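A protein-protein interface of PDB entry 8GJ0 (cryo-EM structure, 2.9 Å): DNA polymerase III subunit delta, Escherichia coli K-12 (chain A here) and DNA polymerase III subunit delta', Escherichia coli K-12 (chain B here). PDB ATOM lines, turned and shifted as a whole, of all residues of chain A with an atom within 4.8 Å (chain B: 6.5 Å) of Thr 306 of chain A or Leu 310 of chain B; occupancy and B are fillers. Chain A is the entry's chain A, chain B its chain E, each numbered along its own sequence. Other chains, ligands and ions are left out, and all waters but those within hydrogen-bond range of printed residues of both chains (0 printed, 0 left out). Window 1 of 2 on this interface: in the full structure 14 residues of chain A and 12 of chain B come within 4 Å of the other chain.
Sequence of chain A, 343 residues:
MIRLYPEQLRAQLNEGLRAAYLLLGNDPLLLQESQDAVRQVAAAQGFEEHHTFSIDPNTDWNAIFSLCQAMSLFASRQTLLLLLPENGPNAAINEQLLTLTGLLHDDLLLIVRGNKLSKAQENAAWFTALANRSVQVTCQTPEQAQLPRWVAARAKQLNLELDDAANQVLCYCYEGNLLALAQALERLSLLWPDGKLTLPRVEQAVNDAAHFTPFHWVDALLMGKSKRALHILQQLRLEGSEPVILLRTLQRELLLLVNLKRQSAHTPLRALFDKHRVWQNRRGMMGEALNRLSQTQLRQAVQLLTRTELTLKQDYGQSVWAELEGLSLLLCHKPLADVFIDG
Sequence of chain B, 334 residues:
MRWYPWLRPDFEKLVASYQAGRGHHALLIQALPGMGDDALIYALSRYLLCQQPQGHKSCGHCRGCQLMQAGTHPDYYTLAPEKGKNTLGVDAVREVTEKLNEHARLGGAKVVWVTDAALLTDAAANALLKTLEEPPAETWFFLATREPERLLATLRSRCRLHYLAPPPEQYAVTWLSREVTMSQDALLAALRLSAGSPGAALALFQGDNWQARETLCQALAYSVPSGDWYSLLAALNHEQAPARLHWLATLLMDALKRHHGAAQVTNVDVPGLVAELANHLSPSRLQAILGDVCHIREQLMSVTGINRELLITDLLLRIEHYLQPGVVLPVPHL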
ATOM      1  N   GLN A 251      -1.433  28.502  23.392  1.00  0.00           N
ATOM      2  CA  GLN A 251      -0.012  28.169  23.365  1.00  0.00           C
ATOM      3  C   GLN A 251       0.798  29.232  22.635  1.00  0.00           C
ATOM      4  O   GLN A 251       1.877  29.625  23.097  1.00  0.00           O
ATOM      5  CB  GLN A 251       0.187  26.803  22.708  1.00  0.00           C
ATOM      6  CG  GLN A 251       1.642  26.369  22.576  1.00  0.00           C
ATOM      7  CD  GLN A 251       1.787  25.038  21.869  1.00  0.00           C
ATOM      8  OE1 GLN A 251       0.821  24.290  21.725  1.00  0.00           O
ATOM      9  NE2 GLN A 251       2.999  24.738  21.419  1.00  0.00           N
ATOM     10  N   LEU A 255       3.749  31.361  24.492  1.00  0.00           N
ATOM     11  CA  LEU A 255       5.144  31.280  24.068  1.00  0.00           C
ATOM     12  C   LEU A 255       5.662  32.643  23.627  1.00  0.00           C
ATOM     13  O   LEU A 255       6.808  33.004  23.919  1.00  0.00           O
ATOM     14  CB  LEU A 255       5.293  30.258  22.942  1.00  0.00           C
ATOM     15  CG  LEU A 255       4.999  28.800  23.306  1.00  0.00           C
ATOM     16  CD1 LEU A 255       5.084  27.917  22.072  1.00  0.00           C
ATOM     17  CD2 LEU A 255       5.948  28.303  24.384  1.00  0.00           C
ATOM     18  N   VAL A 302       3.277  27.217  31.707  1.00  0.00           N
ATOM     19  CA  VAL A 302       3.735  26.206  30.759  1.00  0.00           C
ATOM     20  C   VAL A 302       3.606  24.815  31.365  1.00  0.00           C
ATOM     21  O   VAL A 302       3.210  23.859  30.686  1.00  0.00           O
ATOM     22  CB  VAL A 302       5.181  26.501  30.319  1.00  0.00           C
ATOM     23  CG1 VAL A 302       5.694  25.400  29.405  1.00  0.00           C
ATOM     24  CG2 VAL A 302       5.257  27.850  29.623  1.00  0.00           C
ATOM     25  N   GLN A 303       3.951  24.675  32.647  1.00  0.00           N
ATOM     26  CA  GLN A 303       3.791  23.386  33.313  1.00  0.00           C
ATOM     27  C   GLN A 303       2.328  22.965  33.338  1.00  0.00           C
ATOM     28  O   GLN A 303       2.006  21.799  33.077  1.00  0.00           O
ATOM     29  CB  GLN A 303       4.348  23.455  34.734  1.00  0.00           C
ATOM     30  CG  GLN A 303       5.835  23.746  34.805  1.00  0.00           C
ATOM     31  CD  GLN A 303       6.363  23.716  36.224  1.00  0.00           C
ATOM     32  OE1 GLN A 303       5.631  23.408  37.165  1.00  0.00           O
ATOM     33  NE2 GLN A 303       7.641  24.038  36.388  1.00  0.00           N
ATOM     34  N   LEU A 304       1.428  23.900  33.651  1.00  0.00           N
ATOM     35  CA  LEU A 304       0.005  23.578  33.650  1.00  0.00           C
ATOM     36  C   LEU A 304      -0.456  23.142  32.268  1.00  0.00           C
ATOM     37  O   LEU A 304      -1.205  22.168  32.135  1.00  0.00           O
ATOM     38  CB  LEU A 304      -0.811  24.782  34.119  1.00  0.00           C
ATOM     39  CG  LEU A 304      -0.926  25.016  35.625  1.00  0.00           C
ATOM     40  CD1 LEU A 304      -1.647  26.325  35.891  1.00  0.00           C
ATOM     41  CD2 LEU A 304      -1.654  23.867  36.298  1.00  0.00           C
ATOM     42  N   LEU A 305      -0.025  23.854  31.227  1.00  0.00           N
ATOM     43  CA  LEU A 305      -0.441  23.508  29.874  1.00  0.00           C
ATOM     44  C   LEU A 305       0.067  22.128  29.478  1.00  0.00           C
ATOM     45  O   LEU A 305      -0.677  21.324  28.901  1.00  0.00           O
ATOM     46  CB  LEU A 305       0.058  24.568  28.892  1.00  0.00           C
ATOM     47  CG  LEU A 305      -0.592  24.579  27.506  1.00  0.00           C
ATOM     48  CD1 LEU A 305      -2.039  25.036  27.593  1.00  0.00           C
ATOM     49  CD2 LEU A 305       0.193  25.470  26.559  1.00  0.00           C
ATOM     50  N   THR A 306       1.333  21.832  29.782  1.00  0.00           N
ATOM     51  CA  THR A 306       1.884  20.522  29.452  1.00  0.00           C
ATOM     52  C   THR A 306       1.157  19.413  30.201  1.00  0.00           C
ATOM     53  O   THR A 306       0.825  18.374  29.619  1.00  0.00           O
ATOM     54  CB  THR A 306       3.378  20.483  29.770  1.00  0.00           C
ATOM     55  OG1 THR A 306       3.606  21.007  31.084  1.00  0.00           O
ATOM     56  CG2 THR A 306       4.163  21.293  28.758  1.00  0.00           C
ATOM     57  N   ARG A 307       0.905  19.613  31.498  1.00  0.00           N
ATOM     58  CA  ARG A 307       0.205  18.596  32.272  1.00  0.00           C
ATOM     59  C   ARG A 307      -1.210  18.391  31.745  1.00  0.00           C
ATOM     60  O   ARG A 307      -1.693  17.257  31.671  1.00  0.00           O
ATOM     61  CB  ARG A 307       0.191  18.985  33.751  1.00  0.00           C
ATOM     62  CG  ARG A 307      -0.617  18.054  34.658  1.00  0.00           C
ATOM     63  CD  ARG A 307      -2.085  18.462  34.751  1.00  0.00           C
ATOM     64  NE  ARG A 307      -2.562  18.525  36.127  1.00  0.00           N
ATOM     65  CZ  ARG A 307      -2.281  19.508  36.971  1.00  0.00           C
ATOM     66  NH1 ARG A 307      -1.485  20.508  36.629  1.00  0.00           N
ATOM     67  NH2 ARG A 307      -2.812  19.487  38.190  1.00  0.00           N
ATOM     68  N   THR A 308      -1.890  19.478  31.375  1.00  0.00           N
ATOM     69  CA  THR A 308      -3.236  19.355  30.829  1.00  0.00           C
ATOM     70  C   THR A 308      -3.227  18.591  29.512  1.00  0.00           C
ATOM     71  O   THR A 308      -4.086  17.734  29.280  1.00  0.00           O
ATOM     72  CB  THR A 308      -3.852  20.741  30.638  1.00  0.00           C
ATOM     73  OG1 THR A 308      -3.937  21.408  31.902  1.00  0.00           O
ATOM     74  CG2 THR A 308      -5.241  20.632  30.029  1.00  0.00           C
ATOM     75  N   GLU A 309      -2.265  18.886  28.636  1.00  0.00           N
ATOM     76  CA  GLU A 309      -2.184  18.163  27.371  1.00  0.00           C
ATOM     77  C   GLU A 309      -1.907  16.683  27.602  1.00  0.00           C
ATOM     78  O   GLU A 309      -2.506  15.819  26.949  1.00  0.00           O
ATOM     79  CB  GLU A 309      -1.103  18.780  26.484  1.00  0.00           C
ATOM     80  CG  GLU A 309      -1.047  18.197  25.082  1.00  0.00           C
ATOM     81  CD  GLU A 309      -0.022  18.887  24.206  1.00  0.00           C
ATOM     82  OE1 GLU A 309       0.705  19.765  24.719  1.00  0.00           O
ATOM     83  OE2 GLU A 309       0.059  18.554  23.005  1.00  0.00           O
ATOM     84  N   LEU A 310      -0.997  16.371  28.529  1.00  0.00           N
ATOM     85  CA  LEU A 310      -0.702  14.973  28.825  1.00  0.00           C
ATOM     86  C   LEU A 310      -1.926  14.260  29.384  1.00  0.00           C
ATOM     87  O   LEU A 310      -2.217  13.123  29.003  1.00  0.00           O
ATOM     88  CB  LEU A 310       0.469  14.878  29.803  1.00  0.00           C
ATOM     89  CG  LEU A 310       1.835  15.307  29.263  1.00  0.00           C
ATOM     90  CD1 LEU A 310       2.867  15.310  30.379  1.00  0.00           C
ATOM     91  CD2 LEU A 310       2.282  14.401  28.126  1.00  0.00           C
ATOM     92  N   ASN B 237      14.102  21.730  18.364  1.00  0.00           N
ATOM     93  CA  ASN B 237      12.799  21.666  17.710  1.00  0.00           C
ATOM     94  C   ASN B 237      12.986  21.228  16.262  1.00  0.00           C
ATOM     95  O   ASN B 237      13.450  22.006  15.423  1.00  0.00           O
ATOM     96  CB  ASN B 237      12.106  23.021  17.787  1.00  0.00           C
ATOM     97  CG  ASN B 237      10.645  22.954  17.387  1.00  0.00           C
ATOM     98  OD1 ASN B 237      10.242  22.094  16.604  1.00  0.00           O
ATOM     99  ND2 ASN B 237       9.842  23.864  17.925  1.00  0.00           N
ATOM    100  N   ILE B 306       1.597  14.419  20.233  1.00  0.00           N
ATOM    101  CA  ILE B 306       1.994  15.331  21.295  1.00  0.00           C
ATOM    102  C   ILE B 306       2.737  16.521  20.694  1.00  0.00           C
ATOM    103  O   ILE B 306       3.476  16.394  19.710  1.00  0.00           O
ATOM    104  CB  ILE B 306       2.861  14.601  22.337  1.00  0.00           C
ATOM    105  CG1 ILE B 306       3.101  15.482  23.568  1.00  0.00           C
ATOM    106  CG2 ILE B 306       4.194  14.183  21.729  1.00  0.00           C
ATOM    107  CD1 ILE B 306       1.851  15.790  24.362  1.00  0.00           C
ATOM    108  N   ASN B 307       2.534  17.692  21.293  1.00  0.00           N
ATOM    109  CA  ASN B 307       3.137  18.921  20.794  1.00  0.00           C
ATOM    110  C   ASN B 307       4.621  18.939  21.140  1.00  0.00           C
ATOM    111  O   ASN B 307       4.991  18.953  22.319  1.00  0.00           O
ATOM    112  CB  ASN B 307       2.428  20.137  21.384  1.00  0.00           C
ATOM    113  CG  ASN B 307       2.792  21.423  20.675  1.00  0.00           C
ATOM    114  OD1 ASN B 307       3.762  22.091  21.034  1.00  0.00           O
ATOM    115  ND2 ASN B 307       2.015  21.780  19.661  1.00  0.00           N
ATOM    116  N   ARG B 308       5.467  18.940  20.111  1.00  0.00           N
ATOM    117  CA  ARG B 308       6.909  18.877  20.327  1.00  0.00           C
ATOM    118  C   ARG B 308       7.433  20.159  20.966  1.00  0.00           C
ATOM    119  O   ARG B 308       8.178  20.118  21.955  1.00  0.00           O
ATOM    120  CB  ARG B 308       7.612  18.617  18.994  1.00  0.00           C
ATOM    121  CG  ARG B 308       9.100  18.357  19.104  1.00  0.00           C
ATOM    122  CD  ARG B 308       9.784  18.437  17.747  1.00  0.00           C
ATOM    123  NE  ARG B 308       9.143  17.590  16.747  1.00  0.00           N
ATOM    124  CZ  ARG B 308       8.226  17.997  15.876  1.00  0.00           C
ATOM    125  NH1 ARG B 308       7.802  19.251  15.846  1.00  0.00           N
ATOM    126  NH2 ARG B 308       7.723  17.123  15.010  1.00  0.00           N
ATOM    127  N   GLU B 309       7.053  21.311  20.406  1.00  0.00           N
ATOM    128  CA  GLU B 309       7.634  22.575  20.844  1.00  0.00           C
ATOM    129  C   GLU B 309       7.312  22.856  22.304  1.00  0.00           C
ATOM    130  O   GLU B 309       8.186  23.283  23.068  1.00  0.00           O
ATOM    131  CB  GLU B 309       7.131  23.712  19.957  1.00  0.00           C
ATOM    132  CG  GLU B 309       7.753  25.064  20.266  1.00  0.00           C
ATOM    133  CD  GLU B 309       7.282  26.150  19.320  1.00  0.00           C
ATOM    134  OE1 GLU B 309       6.479  25.843  18.413  1.00  0.00           O
ATOM    135  OE2 GLU B 309       7.714  27.311  19.482  1.00  0.00           O
ATOM    136  N   LEU B 310       6.063  22.630  22.711  1.00  0.00           N
ATOM    137  CA  LEU B 310       5.681  22.903  24.092  1.00  0.00           C
ATOM    138  C   LEU B 310       6.456  22.020  25.061  1.00  0.00           C
ATOM    139  O   LEU B 310       6.949  22.497  26.091  1.00  0.00           O
ATOM    140  CB  LEU B 310       4.176  22.701  24.266  1.00  0.00           C
ATOM    141  CG  LEU B 310       3.605  23.025  25.647  1.00  0.00           C
ATOM    142  CD1 LEU B 310       3.776  24.499  25.977  1.00  0.00           C
ATOM    143  CD2 LEU B 310       2.144  22.621  25.726  1.00  0.00           C
ATOM    144  N   LEU B 311       6.578  20.728  24.747  1.00  0.00           N
ATOM    145  CA  LEU B 311       7.310  19.824  25.626  1.00  0.00           C
ATOM    146  C   LEU B 311       8.775  20.223  25.732  1.00  0.00           C
ATOM    147  O   LEU B 311       9.343  20.237  26.830  1.00  0.00           O
ATOM    148  CB  LEU B 311       7.183  18.385  25.127  1.00  0.00           C
ATOM    149  CG  LEU B 311       6.095  17.547  25.802  1.00  0.00           C
ATOM    150  CD1 LEU B 311       4.729  18.193  25.643  1.00  0.00           C
ATOM    151  CD2 LEU B 311       6.090  16.135  25.241  1.00  0.00           C
ATOM    152  N   ILE B 312       9.407  20.553  24.603  1.00  0.00           N
ATOM    153  CA  ILE B 312      10.819  20.926  24.646  1.00  0.00           C
ATOM    154  C   ILE B 312      11.004  22.218  25.433  1.00  0.00           C
ATOM    155  O   ILE B 312      11.952  22.356  26.218  1.00  0.00           O
ATOM    156  CB  ILE B 312      11.393  21.035  23.221  1.00  0.00           C
ATOM    157  CG1 ILE B 312      11.350  19.664  22.540  1.00  0.00           C
ATOM    158  CG2 ILE B 312      12.827  21.568  23.263  1.00  0.00           C
ATOM    159  CD1 ILE B 312      11.789  19.667  21.090  1.00  0.00           C
ATOM    160  N   THR B 313      10.109  23.190  25.234  1.00  0.00           N
ATOM    161  CA  THR B 313      10.214  24.445  25.970  1.00  0.00           C
ATOM    162  C   THR B 313      10.060  24.216  27.467  1.00  0.00           C
ATOM    163  O   THR B 313      10.810  24.784  28.270  1.00  0.00           O
ATOM    164  CB  THR B 313       9.161  25.435  25.471  1.00  0.00           C
ATOM    165  OG1 THR B 313       9.323  25.641  24.063  1.00  0.00           O
ATOM    166  CG2 THR B 313       9.292  26.767  26.194  1.00  0.00           C
ATOM    167  N   ASP B 314       9.093  23.386  27.863  1.00  0.00           N
ATOM    168  CA  ASP B 314       8.914  23.094  29.280  1.00  0.00           C
ATOM    169  C   ASP B 314      10.137  22.389  29.849  1.00  0.00           C
ATOM    170  O   ASP B 314      10.567  22.681  30.972  1.00  0.00           O
ATOM    171  CB  ASP B 314       7.660  22.244  29.484  1.00  0.00           C
ATOM    172  CG  ASP B 314       7.320  22.048  30.948  1.00  0.00           C
ATOM    173  OD1 ASP B 314       7.987  22.664  31.805  1.00  0.00           O
ATOM    174  OD2 ASP B 314       6.382  21.279  31.242  1.00  0.00           O
ATOM    175  N   LEU B 315      10.710  21.452  29.090  1.00  0.00           N
ATOM    176  CA  LEU B 315      11.911  20.763  29.549  1.00  0.00           C
ATOM    177  C   LEU B 315      13.051  21.747  29.770  1.00  0.00           C
ATOM    178  O   LEU B 315      13.747  21.691  30.789  1.00  0.00           O
ATOM    179  CB  LEU B 315      12.313  19.690  28.534  1.00  0.00           C
ATOM    180  CG  LEU B 315      13.660  18.998  28.763  1.00  0.00           C
ATOM    181  CD1 LEU B 315      13.692  18.313  30.119  1.00  0.00           C
ATOM    182  CD2 LEU B 315      13.944  18.005  27.650  1.00  0.00           C
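Of the 11 printed residues of chain B, 5 touch a printed residue of chain A.
Hydrophobic or aromatic side chains of chain B within 4 Å of the printed part of chain A: Ile 306 and Leu 310.
Of the 11 printed residues of chain A, 7 touch a printed residue of chain B.
Hydrophobic or aromatic side chains of chain A that line the printed part of chain B: Leu 255, Val 302 and Leu 305.
Among the printed residues, 11 pairs touch across the chains.
Of the printed residues of chain B, Gln 303 of chain A touches Asp 314.
Printed residues of chain B within 4 Å of Leu 305 of chain A: Leu 310.
Thr 306 of chain A touches just these residues of chain B: Leu 310 and Asp 314.
The nearest residue of chain B that does not touch Thr 306 of chain A is Leu 311 of chain B (4.4 Å).
The nearest printed residue of chain B that does not touch Leu 255 of chain A is Thr 313 of chain B (4.1 Å).
The backbone NH (N) of Asn 307 of chain B sits at hydrogen-bond distance from the side-chain carboxylate (OE2) of Glu 309 of chain A, 3.1 Å away.
The side-chain hydroxyl (OG1) of Thr 306 of chain A is in hydrogen-bond range of the side-chain carboxylate (OD2) of Asp 314 of chain B, at 2.8 Å.
NE2 of Gln 251 of chain A is in hydrogen-bond range of OD1 of Asn 307 of chain B (2.8 Å).
CB of Leu 310 of chain B touches NE2 of Gln 251 of chain A, at 3.7 Å.
Leu 255 of chain A touches Glu 309 of chain B (CD1 to OE2, 3.7 Å).
Val 302 of chain A touches Asp 314 of chain B (CG1 to CB, 3.7 Å).
Asp 314 of chain B touches Gln 303 of chain A (OD1 to CG, 3.8 Å).
Leu 305 of chain A touches Leu 310 of chain B (CD2 to CD2, 3.6 Å).
Thr 306 of chain A touches Leu 310 of chain B.
Glu 309 of chain A touches Ile 306 of chain B.
Glu 309 of chain A touches Leu 310 of chain B.
OG1 of Thr 313 of chain B sits at hydrogen-bond distance from O of Glu 309 of chain B.
OG1 of Thr 306 of chain A is in hydrogen-bond range of O of Gln 303 of chain A (2.7 Å).
The backbone NH (N) of Glu 309 of chain B lies within hydrogen-bond range of the side-chain amide oxygen (OD1) of Asn 307 of chain B, at 3.4 Å.
OD1 of Asn 307 of chain B sits at hydrogen-bond distance from N of Leu 310 of chain B, at 2.9 Å.
The backbone carbonyl oxygen (O) of Val 302 of chain A sits at hydrogen-bond distance from the side-chain hydroxyl (OG1) of Thr 306 of chain A (2.9 Å).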
